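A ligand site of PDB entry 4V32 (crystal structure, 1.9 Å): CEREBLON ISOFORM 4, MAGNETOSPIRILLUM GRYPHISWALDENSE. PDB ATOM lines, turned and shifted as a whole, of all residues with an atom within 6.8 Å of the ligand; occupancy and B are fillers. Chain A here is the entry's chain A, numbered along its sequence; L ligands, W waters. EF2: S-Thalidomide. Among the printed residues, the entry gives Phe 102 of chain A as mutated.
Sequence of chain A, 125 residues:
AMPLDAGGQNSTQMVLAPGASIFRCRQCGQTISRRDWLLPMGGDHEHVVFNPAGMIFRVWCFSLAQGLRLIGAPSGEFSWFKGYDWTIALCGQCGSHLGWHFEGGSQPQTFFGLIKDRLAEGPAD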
ATOM      1  N   VAL A  49     -12.749  -7.482  21.627  1.00  0.00           N
ATOM      2  CA  VAL A  49     -11.978  -7.557  20.400  1.00  0.00           C
ATOM      3  C   VAL A  49     -11.777  -9.045  20.041  1.00  0.00           C
ATOM      4  O   VAL A  49     -11.910  -9.919  20.907  1.00  0.00           O
ATOM      5  CB  VAL A  49     -10.637  -6.819  20.584  1.00  0.00           C
ATOM      6  CG1 VAL A  49     -10.836  -5.305  20.896  1.00  0.00           C
ATOM      7  CG2 VAL A  49      -9.844  -7.463  21.679  1.00  0.00           C
ATOM      8  N   PHE A  50     -11.434  -9.313  18.793  1.00  0.00           N
ATOM      9  CA  PHE A  50     -11.201 -10.677  18.296  1.00  0.00           C
ATOM     10  C   PHE A  50      -9.804 -10.747  17.694  1.00  0.00           C
ATOM     11  O   PHE A  50      -9.357  -9.794  17.015  1.00  0.00           O
ATOM     12  CB  PHE A  50     -12.221 -10.999  17.202  1.00  0.00           C
ATOM     13  CG  PHE A  50     -13.588 -11.327  17.721  1.00  0.00           C
ATOM     14  CD1 PHE A  50     -13.922 -12.633  18.054  1.00  0.00           C
ATOM     15  CD2 PHE A  50     -14.562 -10.346  17.809  1.00  0.00           C
ATOM     16  CE1 PHE A  50     -15.199 -12.958  18.496  1.00  0.00           C
ATOM     17  CE2 PHE A  50     -15.848 -10.666  18.249  1.00  0.00           C
ATOM     18  CZ  PHE A  50     -16.169 -11.968  18.587  1.00  0.00           C
ATOM     19  N   ASN A  51      -9.102 -11.830  17.937  1.00  0.00           N
ATOM     20  CA  ASN A  51      -7.846 -12.059  17.221  1.00  0.00           C
ATOM     21  C   ASN A  51      -8.031 -12.829  15.897  1.00  0.00           C
ATOM     22  O   ASN A  51      -9.130 -13.236  15.551  1.00  0.00           O
ATOM     23  CB  ASN A  51      -6.817 -12.688  18.191  1.00  0.00           C
ATOM     24  CG  ASN A  51      -7.110 -14.144  18.521  1.00  0.00           C
ATOM     25  OD1 ASN A  51      -8.006 -14.773  17.933  1.00  0.00           O
ATOM     26  ND2 ASN A  51      -6.312 -14.710  19.418  1.00  0.00           N
ATOM     27  N   PRO A  52      -6.960 -12.998  15.111  1.00  0.00           N
ATOM     28  CA  PRO A  52      -7.157 -13.671  13.833  1.00  0.00           C
ATOM     29  C   PRO A  52      -7.587 -15.158  13.944  1.00  0.00           C
ATOM     30  O   PRO A  52      -8.079 -15.673  12.995  1.00  0.00           O
ATOM     31  CB  PRO A  52      -5.790 -13.528  13.133  1.00  0.00           C
ATOM     32  CG  PRO A  52      -5.068 -12.412  13.836  1.00  0.00           C
ATOM     33  CD  PRO A  52      -5.592 -12.433  15.241  1.00  0.00           C
ATOM     34  N   ALA A  53      -7.413 -15.792  15.089  1.00  0.00           N
ATOM     35  CA  ALA A  53      -7.989 -17.128  15.361  1.00  0.00           C
ATOM     36  C   ALA A  53      -9.442 -17.111  15.861  1.00  0.00           C
ATOM     37  O   ALA A  53      -9.966 -18.169  16.273  1.00  0.00           O
ATOM     38  CB  ALA A  53      -7.103 -17.897  16.336  1.00  0.00           C
ATOM     39  N   MET A  55     -10.797 -15.819  18.438  1.00  0.00           N
ATOM     40  CA  MET A  55     -11.002 -15.784  19.889  1.00  0.00           C
ATOM     41  C   MET A  55     -11.417 -14.386  20.283  1.00  0.00           C
ATOM     42  O   MET A  55     -10.783 -13.427  19.856  1.00  0.00           O
ATOM     43  CB  MET A  55      -9.752 -16.154  20.593  1.00  0.00           C
ATOM     44  CG  MET A  55      -9.234 -17.540  20.245  1.00  0.00           C
ATOM     45  SD  MET A  55      -7.708 -17.819  21.127  1.00  0.00           S
ATOM     46  CE  MET A  55      -8.255 -17.612  22.831  1.00  0.00           C
ATOM     47  N   PHE A  57     -12.059 -11.585  23.256  1.00  0.00           N
ATOM     48  CA  PHE A  57     -11.435 -11.152  24.521  1.00  0.00           C
ATOM     49  C   PHE A  57     -12.156  -9.936  25.018  1.00  0.00           C
ATOM     50  O   PHE A  57     -12.411  -8.975  24.278  1.00  0.00           O
ATOM     51  CB  PHE A  57      -9.956 -10.824  24.420  1.00  0.00           C
ATOM     52  CG  PHE A  57      -9.093 -11.919  23.872  1.00  0.00           C
ATOM     53  CD1 PHE A  57      -8.589 -12.924  24.705  1.00  0.00           C
ATOM     54  CD2 PHE A  57      -8.756 -11.952  22.526  1.00  0.00           C
ATOM     55  CE1 PHE A  57      -7.776 -13.912  24.192  1.00  0.00           C
ATOM     56  CE2 PHE A  57      -7.929 -12.929  22.030  1.00  0.00           C
ATOM     57  CZ  PHE A  57      -7.445 -13.911  22.860  1.00  0.00           C
ATOM     58  N   SER A  75       5.157  -5.703  18.311  1.00  0.00           N
ATOM     59  CA  SER A  75       4.669  -5.933  16.966  1.00  0.00           C
ATOM     60  C   SER A  75       3.440  -5.033  16.747  1.00  0.00           C
ATOM     61  O   SER A  75       2.571  -4.909  17.632  1.00  0.00           O
ATOM     62  CB  SER A  75       4.215  -7.394  16.765  1.00  0.00           C
ATOM     63  OG  SER A  75       3.714  -7.524  15.424  1.00  0.00           O
ATOM     64  N   GLY A  76       3.406  -4.409  15.591  1.00  0.00           N
ATOM     65  CA  GLY A  76       2.183  -3.759  15.095  1.00  0.00           C
ATOM     66  C   GLY A  76       1.091  -4.595  14.409  1.00  0.00           C
ATOM     67  O   GLY A  76      -0.016  -4.110  14.187  1.00  0.00           O
ATOM     68  N   GLU A  77       1.352  -5.852  14.077  1.00  0.00           N
ATOM     69  CA  GLU A  77       0.387  -6.649  13.290  1.00  0.00           C
ATOM     70  C   GLU A  77      -0.898  -6.854  14.048  1.00  0.00           C
ATOM     71  O   GLU A  77      -0.887  -7.169  15.230  1.00  0.00           O
ATOM     72  CB  GLU A  77       0.918  -8.039  13.041  1.00  0.00           C
ATOM     73  CG  GLU A  77       2.192  -8.130  12.238  1.00  0.00           C
ATOM     74  CD  GLU A  77       2.522  -9.594  12.061  1.00  0.00           C
ATOM     75  OE1 GLU A  77       1.790 -10.229  11.238  1.00  0.00           O
ATOM     76  OE2 GLU A  77       3.417 -10.117  12.785  1.00  0.00           O
ATOM     77  N   PHE A  78      -2.014  -6.652  13.358  1.00  0.00           N
ATOM     78  CA  PHE A  78      -3.365  -6.860  13.914  1.00  0.00           C
ATOM     79  C   PHE A  78      -3.685  -6.042  15.138  1.00  0.00           C
ATOM     80  O   PHE A  78      -4.657  -6.362  15.827  1.00  0.00           O
ATOM     81  CB  PHE A  78      -3.585  -8.348  14.261  1.00  0.00           C
ATOM     82  CG  PHE A  78      -3.308  -9.290  13.118  1.00  0.00           C
ATOM     83  CD1 PHE A  78      -4.111  -9.292  12.001  1.00  0.00           C
ATOM     84  CD2 PHE A  78      -2.250 -10.176  13.179  1.00  0.00           C
ATOM     85  CE1 PHE A  78      -3.869 -10.141  10.949  1.00  0.00           C
ATOM     86  CE2 PHE A  78      -1.999 -11.045  12.137  1.00  0.00           C
ATOM     87  CZ  PHE A  78      -2.814 -11.044  11.027  1.00  0.00           C
ATOM     88  N   SER A  79      -2.901  -4.992  15.424  1.00  0.00           N
ATOM     89  CA  SER A  79      -3.124  -4.195  16.633  1.00  0.00           C
ATOM     90  C   SER A  79      -4.545  -3.708  16.673  1.00  0.00           C
ATOM     91  O   SER A  79      -5.005  -3.153  15.711  1.00  0.00           O
ATOM     92  CB  SER A  79      -2.216  -2.981  16.732  1.00  0.00           C
ATOM     93  OG  SER A  79      -2.502  -2.333  17.990  1.00  0.00           O
ATOM     94  N   TRP A  80      -5.200  -3.925  17.821  1.00  0.00           N
ATOM     95  CA  TRP A  80      -6.534  -3.440  18.111  1.00  0.00           C
ATOM     96  C   TRP A  80      -6.599  -1.943  18.410  1.00  0.00           C
ATOM     97  O   TRP A  80      -7.668  -1.386  18.435  1.00  0.00           O
ATOM     98  CB  TRP A  80      -7.116  -4.189  19.326  1.00  0.00           C
ATOM     99  CG  TRP A  80      -7.367  -5.654  19.104  1.00  0.00           C
ATOM    100  CD1 TRP A  80      -7.951  -6.224  18.041  1.00  0.00           C
ATOM    101  CD2 TRP A  80      -6.971  -6.715  19.956  1.00  0.00           C
ATOM    102  NE1 TRP A  80      -7.967  -7.603  18.174  1.00  0.00           N
ATOM    103  CE2 TRP A  80      -7.357  -7.929  19.342  1.00  0.00           C
ATOM    104  CE3 TRP A  80      -6.318  -6.767  21.186  1.00  0.00           C
ATOM    105  CZ2 TRP A  80      -7.088  -9.169  19.910  1.00  0.00           C
ATOM    106  CZ3 TRP A  80      -6.060  -7.971  21.735  1.00  0.00           C
ATOM    107  CH2 TRP A  80      -6.474  -9.172  21.125  1.00  0.00           C
ATOM    108  N   PHE A  81      -5.467  -1.274  18.664  1.00  0.00           N
ATOM    109  CA  PHE A  81      -5.516   0.088  19.124  1.00  0.00           C
ATOM    110  C   PHE A  81      -4.627   0.895  18.240  1.00  0.00           C
ATOM    111  O   PHE A  81      -3.472   0.643  18.157  1.00  0.00           O
ATOM    112  CB  PHE A  81      -5.054   0.207  20.557  1.00  0.00           C
ATOM    113  CG  PHE A  81      -5.912  -0.549  21.556  1.00  0.00           C
ATOM    114  CD1 PHE A  81      -7.084   0.046  22.109  1.00  0.00           C
ATOM    115  CD2 PHE A  81      -5.579  -1.783  21.943  1.00  0.00           C
ATOM    116  CE1 PHE A  81      -7.841  -0.643  23.034  1.00  0.00           C
ATOM    117  CE2 PHE A  81      -6.335  -2.472  22.868  1.00  0.00           C
ATOM    118  CZ  PHE A  81      -7.453  -1.906  23.422  1.00  0.00           C
ATOM    119  N   TYR A  84      -0.640   1.838  18.320  1.00  0.00           N
ATOM    120  CA  TYR A  84       0.088   1.007  19.308  1.00  0.00           C
ATOM    121  C   TYR A  84       0.577  -0.304  18.752  1.00  0.00           C
ATOM    122  O   TYR A  84      -0.103  -0.994  17.978  1.00  0.00           O
ATOM    123  CB  TYR A  84      -0.773   0.731  20.593  1.00  0.00           C
ATOM    124  CG  TYR A  84      -1.190   1.952  21.337  1.00  0.00           C
ATOM    125  CD1 TYR A  84      -2.374   2.613  21.025  1.00  0.00           C
ATOM    126  CD2 TYR A  84      -0.405   2.500  22.332  1.00  0.00           C
ATOM    127  CE1 TYR A  84      -2.738   3.797  21.694  1.00  0.00           C
ATOM    128  CE2 TYR A  84      -0.751   3.615  23.005  1.00  0.00           C
ATOM    129  CZ  TYR A  84      -1.967   4.276  22.673  1.00  0.00           C
ATOM    130  OH  TYR A  84      -2.329   5.385  23.350  1.00  0.00           O
ATOM    131  N   TRP A  86       2.301  -4.119  20.208  1.00  0.00           N
ATOM    132  CA  TRP A  86       1.943  -4.941  21.331  1.00  0.00           C
ATOM    133  C   TRP A  86       3.007  -5.977  21.613  1.00  0.00           C
ATOM    134  O   TRP A  86       3.729  -6.419  20.710  1.00  0.00           O
ATOM    135  CB  TRP A  86       0.602  -5.666  21.182  1.00  0.00           C
ATOM    136  CG  TRP A  86       0.442  -6.452  19.970  1.00  0.00           C
ATOM    137  CD1 TRP A  86      -0.201  -6.087  18.842  1.00  0.00           C
ATOM    138  CD2 TRP A  86       0.939  -7.767  19.757  1.00  0.00           C
ATOM    139  NE1 TRP A  86      -0.067  -7.075  17.911  1.00  0.00           N
ATOM    140  CE2 TRP A  86       0.641  -8.105  18.443  1.00  0.00           C
ATOM    141  CE3 TRP A  86       1.650  -8.661  20.537  1.00  0.00           C
ATOM    142  CZ2 TRP A  86       0.990  -9.332  17.889  1.00  0.00           C
ATOM    143  CZ3 TRP A  86       1.974  -9.861  20.012  1.00  0.00           C
ATOM    144  CH2 TRP A  86       1.616 -10.208  18.677  1.00  0.00           C
ATOM    145  N   THR A  87       3.061  -6.308  22.880  1.00  0.00           N
ATOM    146  CA  THR A  87       3.835  -7.456  23.380  1.00  0.00           C
ATOM    147  C   THR A  87       2.926  -8.250  24.291  1.00  0.00           C
ATOM    148  O   THR A  87       2.148  -7.714  25.107  1.00  0.00           O
ATOM    149  CB  THR A  87       5.103  -7.008  24.106  1.00  0.00           C
ATOM    150  OG1 THR A  87       4.741  -6.339  25.280  1.00  0.00           O
ATOM    151  CG2 THR A  87       5.903  -6.032  23.277  1.00  0.00           C
ATOM    152  N   ILE A  88       3.005  -9.563  24.158  1.00  0.00           N
ATOM    153  CA  ILE A  88       2.296 -10.458  25.062  1.00  0.00           C
ATOM    154  C   ILE A  88       2.751 -10.247  26.509  1.00  0.00           C
ATOM    155  O   ILE A  88       3.996 -10.164  26.823  1.00  0.00           O
ATOM    156  CB  ILE A  88       2.533 -11.926  24.589  1.00  0.00           C
ATOM    157  CG1 ILE A  88       1.784 -12.154  23.258  1.00  0.00           C
ATOM    158  CG2 ILE A  88       2.046 -12.920  25.620  1.00  0.00           C
ATOM    159  CD1 ILE A  88       2.259 -13.407  22.484  1.00  0.00           C
ATOM    160  N   HIS A  97      -1.513 -16.456  30.206  1.00  0.00           N
ATOM    161  CA  HIS A  97      -1.546 -15.340  29.298  1.00  0.00           C
ATOM    162  C   HIS A  97      -2.599 -14.375  29.826  1.00  0.00           C
ATOM    163  O   HIS A  97      -3.784 -14.673  29.738  1.00  0.00           O
ATOM    164  CB  HIS A  97      -1.866 -15.779  27.863  1.00  0.00           C
ATOM    165  CG  HIS A  97      -1.980 -14.638  26.901  1.00  0.00           C
ATOM    166  ND1 HIS A  97      -2.792 -14.680  25.774  1.00  0.00           N
ATOM    167  CD2 HIS A  97      -1.493 -13.377  26.949  1.00  0.00           C
ATOM    168  CE1 HIS A  97      -2.712 -13.536  25.130  1.00  0.00           C
ATOM    169  NE2 HIS A  97      -1.958 -12.723  25.843  1.00  0.00           N
ATOM    170  N   TRP A 100      -1.725  -8.080  27.091  1.00  0.00           N
ATOM    171  CA  TRP A 100      -0.678  -7.451  26.247  1.00  0.00           C
ATOM    172  C   TRP A 100      -0.286  -6.108  26.855  1.00  0.00           C
ATOM    173  O   TRP A 100      -1.074  -5.480  27.588  1.00  0.00           O
ATOM    174  CB  TRP A 100      -1.108  -7.284  24.790  1.00  0.00           C
ATOM    175  CG  TRP A 100      -1.733  -8.515  24.139  1.00  0.00           C
ATOM    176  CD1 TRP A 100      -1.090  -9.387  23.305  1.00  0.00           C
ATOM    177  CD2 TRP A 100      -3.045  -9.058  24.308  1.00  0.00           C
ATOM    178  NE1 TRP A 100      -1.878 -10.413  22.991  1.00  0.00           N
ATOM    179  CE2 TRP A 100      -3.109 -10.232  23.569  1.00  0.00           C
ATOM    180  CE3 TRP A 100      -4.191  -8.677  25.033  1.00  0.00           C
ATOM    181  CZ2 TRP A 100      -4.301 -11.047  23.525  1.00  0.00           C
ATOM    182  CZ3 TRP A 100      -5.303  -9.470  25.008  1.00  0.00           C
ATOM    183  CH2 TRP A 100      -5.373 -10.600  24.254  1.00  0.00           C
ATOM    184  N   PHE A 102       0.825  -2.552  25.508  1.00  0.00           N
ATOM    185  CA  PHE A 102       0.784  -1.743  24.340  1.00  0.00           C
ATOM    186  C   PHE A 102       1.706  -0.529  24.486  1.00  0.00           C
ATOM    187  O   PHE A 102       1.759   0.104  25.551  1.00  0.00           O
ATOM    188  CB  PHE A 102      -0.672  -1.270  24.058  1.00  0.00           C
ATOM    189  CG  PHE A 102      -1.593  -2.371  23.613  1.00  0.00           C
ATOM    190  CD1 PHE A 102      -1.621  -2.784  22.318  1.00  0.00           C
ATOM    191  CD2 PHE A 102      -2.355  -3.078  24.565  1.00  0.00           C
ATOM    192  CE1 PHE A 102      -2.479  -3.830  21.892  1.00  0.00           C
ATOM    193  CE2 PHE A 102      -3.134  -4.155  24.181  1.00  0.00           C
ATOM    194  CZ  PHE A 102      -3.234  -4.528  22.838  1.00  0.00           C
HETATM  195  O01 EF2 L   1      -5.102  -9.728  17.398  1.00  0.00           O
HETATM  196  C02 EF2 L   1      -4.302  -9.137  18.277  1.00  0.00           C
HETATM  197  N03 EF2 L   1      -4.231  -7.860  18.324  1.00  0.00           N
HETATM  198  C04 EF2 L   1      -3.654  -7.232  19.299  1.00  0.00           C
HETATM  199  O05 EF2 L   1      -3.833  -5.923  19.390  1.00  0.00           O
HETATM  200  C06 EF2 L   1      -2.794  -7.983  20.333  1.00  0.00           C
HETATM  201  C07 EF2 L   1      -2.300  -9.276  19.749  1.00  0.00           C
HETATM  202  C08 EF2 L   1      -3.513 -10.009  19.256  1.00  0.00           C
HETATM  203  N09 EF2 L   1      -3.182 -11.269  18.584  1.00  0.00           N
HETATM  204  C11 EF2 L   1      -2.700 -15.571  17.081  1.00  0.00           C
HETATM  205  C12 EF2 L   1      -3.222 -14.890  18.153  1.00  0.00           C
HETATM  206  C13 EF2 L   1      -3.104 -13.513  18.147  1.00  0.00           C
HETATM  207  C14 EF2 L   1      -2.491 -12.835  17.090  1.00  0.00           C
HETATM  208  O16 EF2 L   1      -4.214 -12.685  20.230  1.00  0.00           O
HETATM  209  O18 EF2 L   1      -2.034 -10.457  16.603  1.00  0.00           O
HETATM  210  C19 EF2 L   1      -1.969 -13.516  16.017  1.00  0.00           C
HETATM  211  C20 EF2 L   1      -2.064 -14.909  16.038  1.00  0.00           C
HETATM  212  C3  EF2 L   1      -2.580 -11.510  17.413  1.00  0.00           C
HETATM  213  C4  EF2 L   1      -3.509 -12.518  18.983  1.00  0.00           C
HETATM  214  O   HOH W   1       0.442 -11.384  15.319  1.00  0.00           O
HETATM  215  O   HOH W   2      -1.210 -12.476  21.230  1.00  0.00           O
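The side-chain hydroxyl of Ser 79 lies within hydrogen-bond range of the backbone carbonyl oxygen of Phe 81. The side-chain hydroxyl (OG) of Ser 79 lies within hydrogen-bond range of the backbone carbonyl oxygen (O) of Tyr 84, at 2.7 Å. The indole nitrogen of Trp 86 sits at hydrogen-bond distance from the backbone carbonyl oxygen of Glu 77. The side-chain hydroxyl of Ser 75 is in hydrogen-bond range of the backbone NH of Glu 77, 3.2 Å away. The side-chain amide oxygen (OD1) of Asn 51 is in hydrogen-bond range of the backbone NH (N) of Met 55, 3.0 Å away. NE1 of Trp 80 sits at hydrogen-bond distance from O of Phe 50, 2.8 Å away. The side-chain amide oxygen (OD1) of Asn 51 sits at hydrogen-bond distance from the backbone NH (N) of Ala 53, at 3.1 Å. N of Trp 86 lies within hydrogen-bond range of O of Ser 75.
An oxygen (O16) of the ligand is in hydrogen-bond range of the side-chain amide nitrogen of Asn 51, at 3.0 Å. The backbone carbonyl oxygen (O) of Phe 78 lies within hydrogen-bond range of a nitrogen (N03) of the ligand (2.9 Å). O05 of the ligand lies within hydrogen-bond range of N of Trp 80 (2.9 Å).
Merely in contact with the ligand: Pro 52 (3.5 Å), Glu 77 (3.7 Å), Ser 79 (3.3 Å), Trp 86 (3.4 Å), Trp 100 (3.5 Å) and Phe 102 (3.5 Å). Hydrophobic or aromatic side chains that line the ligand: Pro 52, Phe 78, Trp 80, Trp 86, Trp 100 and Phe 102. The nearest printed residue that does not touch the ligand is Phe 57 (4.1 Å).
Water W2 bridges NE1 of Trp 100 (2.8 Å) and O16 of the ligand (3.2 Å).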
